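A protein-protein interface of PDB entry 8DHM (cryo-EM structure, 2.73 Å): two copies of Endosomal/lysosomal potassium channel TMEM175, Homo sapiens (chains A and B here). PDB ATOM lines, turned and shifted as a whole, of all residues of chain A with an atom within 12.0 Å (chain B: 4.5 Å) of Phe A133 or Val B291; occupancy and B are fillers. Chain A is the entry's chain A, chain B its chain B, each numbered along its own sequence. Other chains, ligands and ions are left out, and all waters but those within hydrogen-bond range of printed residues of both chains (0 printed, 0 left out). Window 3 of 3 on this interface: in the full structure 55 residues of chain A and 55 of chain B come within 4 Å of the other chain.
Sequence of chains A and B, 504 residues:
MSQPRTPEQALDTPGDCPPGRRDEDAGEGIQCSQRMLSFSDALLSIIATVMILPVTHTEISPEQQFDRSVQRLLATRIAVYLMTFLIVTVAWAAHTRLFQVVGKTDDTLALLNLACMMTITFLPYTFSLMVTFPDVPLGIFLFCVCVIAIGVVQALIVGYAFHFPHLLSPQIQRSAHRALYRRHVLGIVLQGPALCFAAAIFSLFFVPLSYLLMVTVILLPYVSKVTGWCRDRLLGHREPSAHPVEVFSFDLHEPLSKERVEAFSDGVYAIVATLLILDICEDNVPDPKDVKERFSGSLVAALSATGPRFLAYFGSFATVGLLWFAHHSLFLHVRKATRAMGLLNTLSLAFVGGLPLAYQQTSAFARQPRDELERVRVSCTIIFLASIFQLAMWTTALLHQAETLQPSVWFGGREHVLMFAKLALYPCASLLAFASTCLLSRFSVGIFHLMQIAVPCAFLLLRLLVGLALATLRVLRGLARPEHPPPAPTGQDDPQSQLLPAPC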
ATOM      1  N   THR A  76     -13.427 -28.478   7.215  1.00  0.00           N
ATOM      2  CA  THR A  76     -14.578 -28.271   6.347  1.00  0.00           C
ATOM      3  C   THR A  76     -15.706 -29.218   6.715  1.00  0.00           C
ATOM      4  O   THR A  76     -16.885 -28.873   6.582  1.00  0.00           O
ATOM      5  CB  THR A  76     -14.172 -28.460   4.888  1.00  0.00           C
ATOM      6  OG1 THR A  76     -13.041 -27.634   4.594  1.00  0.00           O
ATOM      7  CG2 THR A  76     -15.312 -28.086   3.963  1.00  0.00           C
ATOM      8  N   VAL A  80     -19.434 -28.098   8.535  1.00  0.00           N
ATOM      9  CA  VAL A  80     -20.672 -28.558   7.923  1.00  0.00           C
ATOM     10  C   VAL A  80     -21.528 -29.286   8.946  1.00  0.00           C
ATOM     11  O   VAL A  80     -22.761 -29.198   8.918  1.00  0.00           O
ATOM     12  CB  VAL A  80     -20.364 -29.438   6.701  1.00  0.00           C
ATOM     13  CG1 VAL A  80     -21.600 -30.183   6.252  1.00  0.00           C
ATOM     14  CG2 VAL A  80     -19.823 -28.589   5.582  1.00  0.00           C
ATOM     15  N   PRO A 124     -29.865 -31.886   5.405  1.00  0.00           N
ATOM     16  CA  PRO A 124     -28.403 -32.046   5.427  1.00  0.00           C
ATOM     17  C   PRO A 124     -27.797 -32.279   4.058  1.00  0.00           C
ATOM     18  O   PRO A 124     -26.762 -31.682   3.733  1.00  0.00           O
ATOM     19  CB  PRO A 124     -28.203 -33.253   6.352  1.00  0.00           C
ATOM     20  CG  PRO A 124     -29.424 -33.329   7.147  1.00  0.00           C
ATOM     21  CD  PRO A 124     -30.523 -32.855   6.295  1.00  0.00           C
ATOM     22  N   TYR A 125     -28.415 -33.132   3.240  1.00  0.00           N
ATOM     23  CA  TYR A 125     -27.873 -33.410   1.916  1.00  0.00           C
ATOM     24  C   TYR A 125     -27.860 -32.160   1.051  1.00  0.00           C
ATOM     25  O   TYR A 125     -26.859 -31.865   0.392  1.00  0.00           O
ATOM     26  CB  TYR A 125     -28.680 -34.521   1.250  1.00  0.00           C
ATOM     27  CG  TYR A 125     -28.224 -34.850  -0.149  1.00  0.00           C
ATOM     28  CD1 TYR A 125     -28.778 -34.216  -1.249  1.00  0.00           C
ATOM     29  CD2 TYR A 125     -27.229 -35.783  -0.368  1.00  0.00           C
ATOM     30  CE1 TYR A 125     -28.360 -34.508  -2.516  1.00  0.00           C
ATOM     31  CE2 TYR A 125     -26.805 -36.081  -1.633  1.00  0.00           C
ATOM     32  CZ  TYR A 125     -27.372 -35.440  -2.705  1.00  0.00           C
ATOM     33  OH  TYR A 125     -26.948 -35.740  -3.973  1.00  0.00           O
ATOM     34  N   THR A 126     -28.957 -31.408   1.049  1.00  0.00           N
ATOM     35  CA  THR A 126     -29.042 -30.197   0.249  1.00  0.00           C
ATOM     36  C   THR A 126     -28.092 -29.113   0.726  1.00  0.00           C
ATOM     37  O   THR A 126     -27.515 -28.406  -0.103  1.00  0.00           O
ATOM     38  CB  THR A 126     -30.474 -29.671   0.251  1.00  0.00           C
ATOM     39  OG1 THR A 126     -30.938 -29.531   1.598  1.00  0.00           O
ATOM     40  CG2 THR A 126     -31.379 -30.615  -0.500  1.00  0.00           C
ATOM     41  N   PHE A 127     -27.909 -28.969   2.035  1.00  0.00           N
ATOM     42  CA  PHE A 127     -26.955 -28.007   2.564  1.00  0.00           C
ATOM     43  C   PHE A 127     -25.516 -28.379   2.220  1.00  0.00           C
ATOM     44  O   PHE A 127     -24.724 -27.510   1.830  1.00  0.00           O
ATOM     45  CB  PHE A 127     -27.136 -27.894   4.077  1.00  0.00           C
ATOM     46  CG  PHE A 127     -26.197 -26.931   4.729  1.00  0.00           C
ATOM     47  CD1 PHE A 127     -26.485 -25.582   4.759  1.00  0.00           C
ATOM     48  CD2 PHE A 127     -25.032 -27.374   5.320  1.00  0.00           C
ATOM     49  CE1 PHE A 127     -25.630 -24.695   5.355  1.00  0.00           C
ATOM     50  CE2 PHE A 127     -24.171 -26.489   5.918  1.00  0.00           C
ATOM     51  CZ  PHE A 127     -24.470 -25.148   5.937  1.00  0.00           C
ATOM     52  N   SER A 128     -25.163 -29.659   2.352  1.00  0.00           N
ATOM     53  CA  SER A 128     -23.837 -30.105   1.944  1.00  0.00           C
ATOM     54  C   SER A 128     -23.618 -29.895   0.453  1.00  0.00           C
ATOM     55  O   SER A 128     -22.523 -29.508   0.033  1.00  0.00           O
ATOM     56  CB  SER A 128     -23.651 -31.573   2.314  1.00  0.00           C
ATOM     57  OG  SER A 128     -22.288 -31.958   2.254  1.00  0.00           O
ATOM     58  N   LEU A 129     -24.644 -30.148  -0.356  1.00  0.00           N
ATOM     59  CA  LEU A 129     -24.568 -29.898  -1.788  1.00  0.00           C
ATOM     60  C   LEU A 129     -24.367 -28.418  -2.090  1.00  0.00           C
ATOM     61  O   LEU A 129     -23.585 -28.063  -2.979  1.00  0.00           O
ATOM     62  CB  LEU A 129     -25.844 -30.413  -2.450  1.00  0.00           C
ATOM     63  CG  LEU A 129     -25.847 -30.696  -3.946  1.00  0.00           C
ATOM     64  CD1 LEU A 129     -26.887 -31.751  -4.214  1.00  0.00           C
ATOM     65  CD2 LEU A 129     -26.127 -29.458  -4.754  1.00  0.00           C
ATOM     66  N   MET A 130     -25.070 -27.545  -1.370  1.00  0.00           N
ATOM     67  CA  MET A 130     -24.939 -26.109  -1.581  1.00  0.00           C
ATOM     68  C   MET A 130     -23.567 -25.588  -1.181  1.00  0.00           C
ATOM     69  O   MET A 130     -23.036 -24.700  -1.855  1.00  0.00           O
ATOM     70  CB  MET A 130     -26.028 -25.368  -0.803  1.00  0.00           C
ATOM     71  CG  MET A 130     -25.958 -23.858  -0.904  1.00  0.00           C
ATOM     72  SD  MET A 130     -27.341 -23.032  -0.097  1.00  0.00           S
ATOM     73  CE  MET A 130     -26.985 -23.375   1.622  1.00  0.00           C
ATOM     74  N   VAL A 131     -22.983 -26.110  -0.105  1.00  0.00           N
ATOM     75  CA  VAL A 131     -21.658 -25.651   0.300  1.00  0.00           C
ATOM     76  C   VAL A 131     -20.548 -26.292  -0.531  1.00  0.00           C
ATOM     77  O   VAL A 131     -19.467 -25.711  -0.662  1.00  0.00           O
ATOM     78  CB  VAL A 131     -21.429 -25.898   1.802  1.00  0.00           C
ATOM     79  CG1 VAL A 131     -22.518 -25.230   2.620  1.00  0.00           C
ATOM     80  CG2 VAL A 131     -21.343 -27.382   2.105  1.00  0.00           C
ATOM     81  N   THR A 132     -20.785 -27.478  -1.097  1.00  0.00           N
ATOM     82  CA  THR A 132     -19.758 -28.129  -1.904  1.00  0.00           C
ATOM     83  C   THR A 132     -19.655 -27.501  -3.290  1.00  0.00           C
ATOM     84  O   THR A 132     -18.565 -27.442  -3.869  1.00  0.00           O
ATOM     85  CB  THR A 132     -20.055 -29.622  -2.013  1.00  0.00           C
ATOM     86  OG1 THR A 132     -20.015 -30.212  -0.711  1.00  0.00           O
ATOM     87  CG2 THR A 132     -19.038 -30.304  -2.898  1.00  0.00           C
ATOM     88  N   PHE A 133     -20.775 -27.031  -3.837  1.00  0.00           N
ATOM     89  CA  PHE A 133     -20.824 -26.389  -5.148  1.00  0.00           C
ATOM     90  C   PHE A 133     -21.368 -24.977  -4.972  1.00  0.00           C
ATOM     91  O   PHE A 133     -22.517 -24.689  -5.331  1.00  0.00           O
ATOM     92  CB  PHE A 133     -21.692 -27.173  -6.130  1.00  0.00           C
ATOM     93  CG  PHE A 133     -21.234 -28.579  -6.356  1.00  0.00           C
ATOM     94  CD1 PHE A 133     -21.576 -29.578  -5.470  1.00  0.00           C
ATOM     95  CD2 PHE A 133     -20.470 -28.903  -7.458  1.00  0.00           C
ATOM     96  CE1 PHE A 133     -21.160 -30.867  -5.674  1.00  0.00           C
ATOM     97  CE2 PHE A 133     -20.054 -30.190  -7.665  1.00  0.00           C
ATOM     98  CZ  PHE A 133     -20.400 -31.175  -6.772  1.00  0.00           C
ATOM     99  N   PRO A 134     -20.566 -24.071  -4.413  1.00  0.00           N
ATOM    100  CA  PRO A 134     -21.072 -22.713  -4.170  1.00  0.00           C
ATOM    101  C   PRO A 134     -21.481 -21.979  -5.433  1.00  0.00           C
ATOM    102  O   PRO A 134     -22.492 -21.265  -5.428  1.00  0.00           O
ATOM    103  CB  PRO A 134     -19.893 -22.036  -3.467  1.00  0.00           C
ATOM    104  CG  PRO A 134     -18.703 -22.765  -3.943  1.00  0.00           C
ATOM    105  CD  PRO A 134     -19.127 -24.184  -4.132  1.00  0.00           C
ATOM    106  N   ASP A 135     -20.728 -22.134  -6.523  1.00  0.00           N
ATOM    107  CA  ASP A 135     -21.026 -21.388  -7.740  1.00  0.00           C
ATOM    108  C   ASP A 135     -22.231 -21.950  -8.480  1.00  0.00           C
ATOM    109  O   ASP A 135     -22.976 -21.188  -9.105  1.00  0.00           O
ATOM    110  CB  ASP A 135     -19.805 -21.378  -8.659  1.00  0.00           C
ATOM    111  CG  ASP A 135     -18.655 -20.570  -8.092  1.00  0.00           C
ATOM    112  OD1 ASP A 135     -18.914 -19.617  -7.328  1.00  0.00           O
ATOM    113  OD2 ASP A 135     -17.490 -20.889  -8.410  1.00  0.00           O
ATOM    114  N   VAL A 136     -22.438 -23.258  -8.431  1.00  0.00           N
ATOM    115  CA  VAL A 136     -23.582 -23.864  -9.120  1.00  0.00           C
ATOM    116  C   VAL A 136     -24.873 -23.386  -8.462  1.00  0.00           C
ATOM    117  O   VAL A 136     -25.001 -23.470  -7.228  1.00  0.00           O
ATOM    118  CB  VAL A 136     -23.476 -25.387  -9.084  1.00  0.00           C
ATOM    119  CG1 VAL A 136     -24.719 -26.022  -9.675  1.00  0.00           C
ATOM    120  CG2 VAL A 136     -22.246 -25.844  -9.835  1.00  0.00           C
ATOM    121  N   PRO A 137     -25.851 -22.882  -9.224  1.00  0.00           N
ATOM    122  CA  PRO A 137     -27.082 -22.377  -8.598  1.00  0.00           C
ATOM    123  C   PRO A 137     -28.058 -23.456  -8.166  1.00  0.00           C
ATOM    124  O   PRO A 137     -29.005 -23.146  -7.432  1.00  0.00           O
ATOM    125  CB  PRO A 137     -27.690 -21.503  -9.701  1.00  0.00           C
ATOM    126  CG  PRO A 137     -27.243 -22.150 -10.947  1.00  0.00           C
ATOM    127  CD  PRO A 137     -25.851 -22.645 -10.677  1.00  0.00           C
ATOM    128  N   LEU A 138     -27.866 -24.703  -8.596  1.00  0.00           N
ATOM    129  CA  LEU A 138     -28.837 -25.750  -8.299  1.00  0.00           C
ATOM    130  C   LEU A 138     -28.900 -26.065  -6.807  1.00  0.00           C
ATOM    131  O   LEU A 138     -29.970 -26.409  -6.293  1.00  0.00           O
ATOM    132  CB  LEU A 138     -28.497 -27.005  -9.104  1.00  0.00           C
ATOM    133  CG  LEU A 138     -29.295 -28.284  -8.847  1.00  0.00           C
ATOM    134  CD1 LEU A 138     -30.687 -28.179  -9.426  1.00  0.00           C
ATOM    135  CD2 LEU A 138     -28.573 -29.470  -9.450  1.00  0.00           C
ATOM    136  N   GLY A 139     -27.774 -25.965  -6.099  1.00  0.00           N
ATOM    137  CA  GLY A 139     -27.770 -26.321  -4.688  1.00  0.00           C
ATOM    138  C   GLY A 139     -28.614 -25.389  -3.842  1.00  0.00           C
ATOM    139  O   GLY A 139     -29.378 -25.835  -2.978  1.00  0.00           O
ATOM    140  N   ILE A 140     -28.482 -24.083  -4.072  1.00  0.00           N
ATOM    141  CA  ILE A 140     -29.320 -23.118  -3.376  1.00  0.00           C
ATOM    142  C   ILE A 140     -30.786 -23.391  -3.678  1.00  0.00           C
ATOM    143  O   ILE A 140     -31.642 -23.351  -2.785  1.00  0.00           O
ATOM    144  CB  ILE A 140     -28.911 -21.689  -3.775  1.00  0.00           C
ATOM    145  CG1 ILE A 140     -27.445 -21.434  -3.429  1.00  0.00           C
ATOM    146  CG2 ILE A 140     -29.779 -20.668  -3.070  1.00  0.00           C
ATOM    147  CD1 ILE A 140     -26.875 -20.177  -4.059  1.00  0.00           C
ATOM    148  N   PHE A 141     -31.094 -23.682  -4.942  1.00  0.00           N
ATOM    149  CA  PHE A 141     -32.468 -23.957  -5.343  1.00  0.00           C
ATOM    150  C   PHE A 141     -33.033 -25.160  -4.597  1.00  0.00           C
ATOM    151  O   PHE A 141     -34.156 -25.108  -4.083  1.00  0.00           O
ATOM    152  CB  PHE A 141     -32.509 -24.178  -6.855  1.00  0.00           C
ATOM    153  CG  PHE A 141     -33.835 -24.638  -7.373  1.00  0.00           C
ATOM    154  CD1 PHE A 141     -34.022 -25.954  -7.756  1.00  0.00           C
ATOM    155  CD2 PHE A 141     -34.888 -23.755  -7.502  1.00  0.00           C
ATOM    156  CE1 PHE A 141     -35.233 -26.378  -8.242  1.00  0.00           C
ATOM    157  CE2 PHE A 141     -36.101 -24.176  -7.988  1.00  0.00           C
ATOM    158  CZ  PHE A 141     -36.274 -25.489  -8.359  1.00  0.00           C
ATOM    159  N   LEU A 142     -32.263 -26.244  -4.507  1.00  0.00           N
ATOM    160  CA  LEU A 142     -32.747 -27.446  -3.837  1.00  0.00           C
ATOM    161  C   LEU A 142     -32.894 -27.251  -2.331  1.00  0.00           C
ATOM    162  O   LEU A 142     -33.862 -27.743  -1.735  1.00  0.00           O
ATOM    163  CB  LEU A 142     -31.814 -28.616  -4.137  1.00  0.00           C
ATOM    164  CG  LEU A 142     -31.721 -29.021  -5.610  1.00  0.00           C
ATOM    165  CD1 LEU A 142     -30.584 -29.991  -5.843  1.00  0.00           C
ATOM    166  CD2 LEU A 142     -33.024 -29.617  -6.090  1.00  0.00           C
ATOM    167  N   PHE A 143     -31.962 -26.534  -1.700  1.00  0.00           N
ATOM    168  CA  PHE A 143     -32.099 -26.241  -0.276  1.00  0.00           C
ATOM    169  C   PHE A 143     -33.336 -25.388  -0.004  1.00  0.00           C
ATOM    170  O   PHE A 143     -34.100 -25.656   0.941  1.00  0.00           O
ATOM    171  CB  PHE A 143     -30.832 -25.548   0.218  1.00  0.00           C
ATOM    172  CG  PHE A 143     -30.835 -25.231   1.679  1.00  0.00           C
ATOM    173  CD1 PHE A 143     -30.737 -26.238   2.616  1.00  0.00           C
ATOM    174  CD2 PHE A 143     -30.912 -23.924   2.117  1.00  0.00           C
ATOM    175  CE1 PHE A 143     -30.733 -25.951   3.957  1.00  0.00           C
ATOM    176  CE2 PHE A 143     -30.909 -23.635   3.458  1.00  0.00           C
ATOM    177  CZ  PHE A 143     -30.817 -24.647   4.378  1.00  0.00           C
ATOM    178  N   CYS A 144     -33.562 -24.369  -0.835  1.00  0.00           N
ATOM    179  CA  CYS A 144     -34.749 -23.540  -0.677  1.00  0.00           C
ATOM    180  C   CYS A 144     -36.016 -24.356  -0.878  1.00  0.00           C
ATOM    181  O   CYS A 144     -37.007 -24.152  -0.174  1.00  0.00           O
ATOM    182  CB  CYS A 144     -34.708 -22.369  -1.655  1.00  0.00           C
ATOM    183  SG  CYS A 144     -33.468 -21.115  -1.268  1.00  0.00           S
ATOM    184  N   PRO B 286     -22.135 -35.528  -4.825  1.00  0.00           N
ATOM    185  CA  PRO B 286     -21.200 -35.490  -5.953  1.00  0.00           C
ATOM    186  C   PRO B 286     -19.947 -34.686  -5.642  1.00  0.00           C
ATOM    187  O   PRO B 286     -19.994 -33.643  -4.988  1.00  0.00           O
ATOM    188  CB  PRO B 286     -22.024 -34.841  -7.069  1.00  0.00           C
ATOM    189  CG  PRO B 286     -23.412 -35.132  -6.721  1.00  0.00           C
ATOM    190  CD  PRO B 286     -23.479 -35.085  -5.233  1.00  0.00           C
ATOM    191  N   ASP B 287     -18.826 -35.192  -6.117  1.00  0.00           N
ATOM    192  CA  ASP B 287     -17.520 -34.548  -6.044  1.00  0.00           C
ATOM    193  C   ASP B 287     -17.364 -33.564  -7.197  1.00  0.00           C
ATOM    194  O   ASP B 287     -17.638 -33.927  -8.348  1.00  0.00           O
ATOM    195  CB  ASP B 287     -16.414 -35.589  -6.110  1.00  0.00           C
ATOM    196  CG  ASP B 287     -15.086 -35.074  -5.597  1.00  0.00           C
ATOM    197  OD1 ASP B 287     -14.986 -33.874  -5.282  1.00  0.00           O
ATOM    198  OD2 ASP B 287     -14.134 -35.878  -5.506  1.00  0.00           O
ATOM    199  N   PRO B 288     -16.947 -32.319  -6.946  1.00  0.00           N
ATOM    200  CA  PRO B 288     -16.631 -31.426  -8.072  1.00  0.00           C
ATOM    201  C   PRO B 288     -15.702 -32.070  -9.087  1.00  0.00           C
ATOM    202  O   PRO B 288     -15.813 -31.818 -10.294  1.00  0.00           O
ATOM    203  CB  PRO B 288     -15.982 -30.225  -7.376  1.00  0.00           C
ATOM    204  CG  PRO B 288     -16.597 -30.199  -6.035  1.00  0.00           C
ATOM    205  CD  PRO B 288     -16.867 -31.618  -5.652  1.00  0.00           C
ATOM    206  N   LYS B 289     -14.791 -32.917  -8.611  1.00  0.00           N
ATOM    207  CA  LYS B 289     -13.892 -33.654  -9.491  1.00  0.00           C
ATOM    208  C   LYS B 289     -14.660 -34.573 -10.435  1.00  0.00           C
ATOM    209  O   LYS B 289     -14.479 -34.512 -11.659  1.00  0.00           O
ATOM    210  CB  LYS B 289     -12.926 -34.456  -8.621  1.00  0.00           C
ATOM    211  CG  LYS B 289     -11.865 -35.263  -9.342  1.00  0.00           C
ATOM    212  CD  LYS B 289     -10.902 -34.413 -10.156  1.00  0.00           C
ATOM    213  CE  LYS B 289     -10.061 -33.507  -9.265  1.00  0.00           C
ATOM    214  NZ  LYS B 289      -9.108 -34.270  -8.414  1.00  0.00           N
ATOM    215  N   ASP B 290     -15.530 -35.422  -9.884  1.00  0.00           N
ATOM    216  CA  ASP B 290     -16.307 -36.332 -10.716  1.00  0.00           C
ATOM    217  C   ASP B 290     -17.221 -35.559 -11.654  1.00  0.00           C
ATOM    218  O   ASP B 290     -17.430 -35.959 -12.804  1.00  0.00           O
ATOM    219  CB  ASP B 290     -17.114 -37.280  -9.831  1.00  0.00           C
ATOM    220  CG  ASP B 290     -17.659 -38.470 -10.592  1.00  0.00           C
ATOM    221  OD1 ASP B 290     -18.150 -38.279 -11.723  1.00  0.00           O
ATOM    222  OD2 ASP B 290     -17.593 -39.598 -10.063  1.00  0.00           O
ATOM    223  N   VAL B 291     -17.773 -34.442 -11.175  1.00  0.00           N
ATOM    224  CA  VAL B 291     -18.626 -33.610 -12.006  1.00  0.00           C
ATOM    225  C   VAL B 291     -17.856 -33.014 -13.173  1.00  0.00           C
ATOM    226  O   VAL B 291     -18.414 -32.859 -14.264  1.00  0.00           O
ATOM    227  CB  VAL B 291     -19.265 -32.509 -11.144  1.00  0.00           C
ATOM    228  CG1 VAL B 291     -19.958 -31.483 -12.012  1.00  0.00           C
ATOM    229  CG2 VAL B 291     -20.231 -33.124 -10.150  1.00  0.00           C
ATOM    230  N   LYS B 292     -16.586 -32.668 -12.973  1.00  0.00           N
ATOM    231  CA  LYS B 292     -15.767 -32.106 -14.035  1.00  0.00           C
ATOM    232  C   LYS B 292     -15.165 -33.159 -14.954  1.00  0.00           C
ATOM    233  O   LYS B 292     -14.743 -32.815 -16.064  1.00  0.00           O
ATOM    234  CB  LYS B 292     -14.639 -31.259 -13.434  1.00  0.00           C
ATOM    235  CG  LYS B 292     -13.729 -30.619 -14.464  1.00  0.00           C
ATOM    236  CD  LYS B 292     -12.808 -29.595 -13.829  1.00  0.00           C
ATOM    237  CE  LYS B 292     -11.901 -28.955 -14.863  1.00  0.00           C
ATOM    238  NZ  LYS B 292     -10.954 -27.984 -14.252  1.00  0.00           N
ATOM    239  N   GLU B 293     -15.119 -34.423 -14.537  1.00  0.00           N
ATOM    240  CA  GLU B 293     -14.483 -35.472 -15.329  1.00  0.00           C
ATOM    241  C   GLU B 293     -15.460 -36.392 -16.043  1.00  0.00           C
ATOM    242  O   GLU B 293     -15.276 -36.668 -17.230  1.00  0.00           O
ATOM    243  CB  GLU B 293     -13.567 -36.320 -14.440  1.00  0.00           C
ATOM    244  CG  GLU B 293     -12.227 -35.674 -14.147  1.00  0.00           C
ATOM    245  CD  GLU B 293     -11.238 -36.643 -13.530  1.00  0.00           C
ATOM    246  OE1 GLU B 293     -11.665 -37.497 -12.726  1.00  0.00           O
ATOM    247  OE2 GLU B 293     -10.034 -36.550 -13.849  1.00  0.00           O
ATOM    248  N   PHE B 295     -19.174 -36.214 -15.861  1.00  0.00           N
ATOM    249  CA  PHE B 295     -20.511 -35.711 -16.145  1.00  0.00           C
ATOM    250  C   PHE B 295     -20.496 -34.396 -16.915  1.00  0.00           C
ATOM    251  O   PHE B 295     -21.535 -33.734 -17.009  1.00  0.00           O
ATOM    252  CB  PHE B 295     -21.299 -35.550 -14.846  1.00  0.00           C
ATOM    253  CG  PHE B 295     -21.487 -36.831 -14.089  1.00  0.00           C
ATOM    254  CD1 PHE B 295     -22.304 -37.828 -14.585  1.00  0.00           C
ATOM    255  CD2 PHE B 295     -20.849 -37.037 -12.882  1.00  0.00           C
ATOM    256  CE1 PHE B 295     -22.479 -39.003 -13.891  1.00  0.00           C
ATOM    257  CE2 PHE B 295     -21.023 -38.212 -12.183  1.00  0.00           C
ATOM    258  CZ  PHE B 295     -21.835 -39.195 -12.686  1.00  0.00           C
ATOM    259  N   SER B 296     -19.352 -34.003 -17.468  1.00  0.00           N
ATOM    260  CA  SER B 296     -19.229 -32.853 -18.360  1.00  0.00           C
ATOM    261  C   SER B 296     -19.487 -31.523 -17.662  1.00  0.00           C
ATOM    262  O   SER B 296     -19.710 -30.511 -18.338  1.00  0.00           O
ATOM    263  CB  SER B 296     -20.167 -32.993 -19.563  1.00  0.00           C
ATOM    264  OG  SER B 296     -19.781 -32.125 -20.613  1.00  0.00           O
ATOM    265  N   GLY B 297     -19.462 -31.489 -16.332  1.00  0.00           N
ATOM    266  CA  GLY B 297     -19.625 -30.262 -15.579  1.00  0.00           C
ATOM    267  C   GLY B 297     -21.023 -30.016 -15.061  1.00  0.00           C
ATOM    268  O   GLY B 297     -21.205 -29.121 -14.226  1.00  0.00           O
ATOM    269  N   SER B 298     -22.013 -30.770 -15.524  1.00  0.00           N
ATOM    270  CA  SER B 298     -23.383 -30.591 -15.067  1.00  0.00           C
ATOM    271  C   SER B 298     -23.612 -31.392 -13.795  1.00  0.00           C
ATOM    272  O   SER B 298     -23.562 -32.626 -13.814  1.00  0.00           O
ATOM    273  CB  SER B 298     -24.366 -31.029 -16.148  1.00  0.00           C
ATOM    274  OG  SER B 298     -24.115 -32.366 -16.538  1.00  0.00           O
ATOM    275  N   LEU B 299     -23.863 -30.692 -12.691  1.00  0.00           N
ATOM    276  CA  LEU B 299     -24.233 -31.359 -11.453  1.00  0.00           C
ATOM    277  C   LEU B 299     -25.614 -31.986 -11.536  1.00  0.00           C
ATOM    278  O   LEU B 299     -25.893 -32.943 -10.806  1.00  0.00           O
ATOM    279  CB  LEU B 299     -24.164 -30.368 -10.290  1.00  0.00           C
ATOM    280  CG  LEU B 299     -24.605 -30.879  -8.923  1.00  0.00           C
ATOM    281  CD1 LEU B 299     -23.646 -31.916  -8.413  1.00  0.00           C
ATOM    282  CD2 LEU B 299     -24.679 -29.732  -7.964  1.00  0.00           C
ATOM    283  N   ALA B 302     -24.857 -35.461 -12.699  1.00  0.00           N
ATOM    284  CA  ALA B 302     -24.254 -36.246 -11.629  1.00  0.00           C
ATOM    285  C   ALA B 302     -25.281 -36.640 -10.578  1.00  0.00           C
ATOM    286  O   ALA B 302     -25.159 -37.706  -9.963  1.00  0.00           O
ATOM    287  CB  ALA B 302     -23.118 -35.464 -10.983  1.00  0.00           C
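Val B291 touches one residue of chain A.
Of chain A, only Tyr A125 (3.7 Å) and Phe A133 (3.1 Å) come within 4 Å of Pro B286.
Asp B287 touches just one residue of chain A: Phe A133 (3.9 Å).
Phe B295 touches none of the printed residues of chain A.
Gly B297 touches none of the printed residues of chain A.
No residue of chain A comes within 4 Å of Ala B302.
Printed residues of chain B within 4 Å of Thr A132: Pro B288 (3.7 Å).
Of the printed residues of chain B, Leu A129 touches Leu B299.
Printed residues of chain B within 4 Å of Tyr A125: Pro B286.
Phe A143 touches none of the printed residues of chain B.
Phe A127 touches none of the printed residues of chain B.
The nearest printed residue of chain B that does not touch Phe A133 is Lys B289 (6.0 Å).
The nearest residue of chain A that does not touch Val B291 is Val A136 (6.5 Å).
The nearest printed residue of chain B that does not touch Tyr A125 is Ala B302 (6.6 Å).
No position is printed for both chains.
Of the 8 pairs that touch across the chains among the printed residues, none has its exchanged pair printed and touching as well.
Of the 23 printed residues of chain A, 4 touch a printed residue of chain B.
Among the printed residues, 8 pairs touch across the chains.
Among the printed residues, no Asp or Glu carboxylate lies within 4 Å of a Lys or Arg side-chain nitrogen of the other chain.
Among the printed residues, merely in contact across the chains: Tyr A125 with Pro B286 (3.7 Å), Leu A129 with Leu B299 (3.5 Å), Thr A132 with Pro B288 (3.7 Å), Phe A133 with Pro B286 (3.1 Å), Phe A133 with Asp B287 (3.9 Å), Phe A133 with Pro B288 (3.6 Å), Phe A133 with Val B291 (3.8 Å) and Phe A133 with Leu B299 (3.7 Å).
The side-chain carboxylate (OD1) of Asp B287 lies close to the backbone NH (N) of Lys B289 (3.5 Å).
The backbone NH (N) of Gly B297 is in hydrogen-bond range of the backbone carbonyl oxygen (O) of Val B291 (2.7 Å).
O of Ser A128 is in hydrogen-bond range of OG1 of Thr A132.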
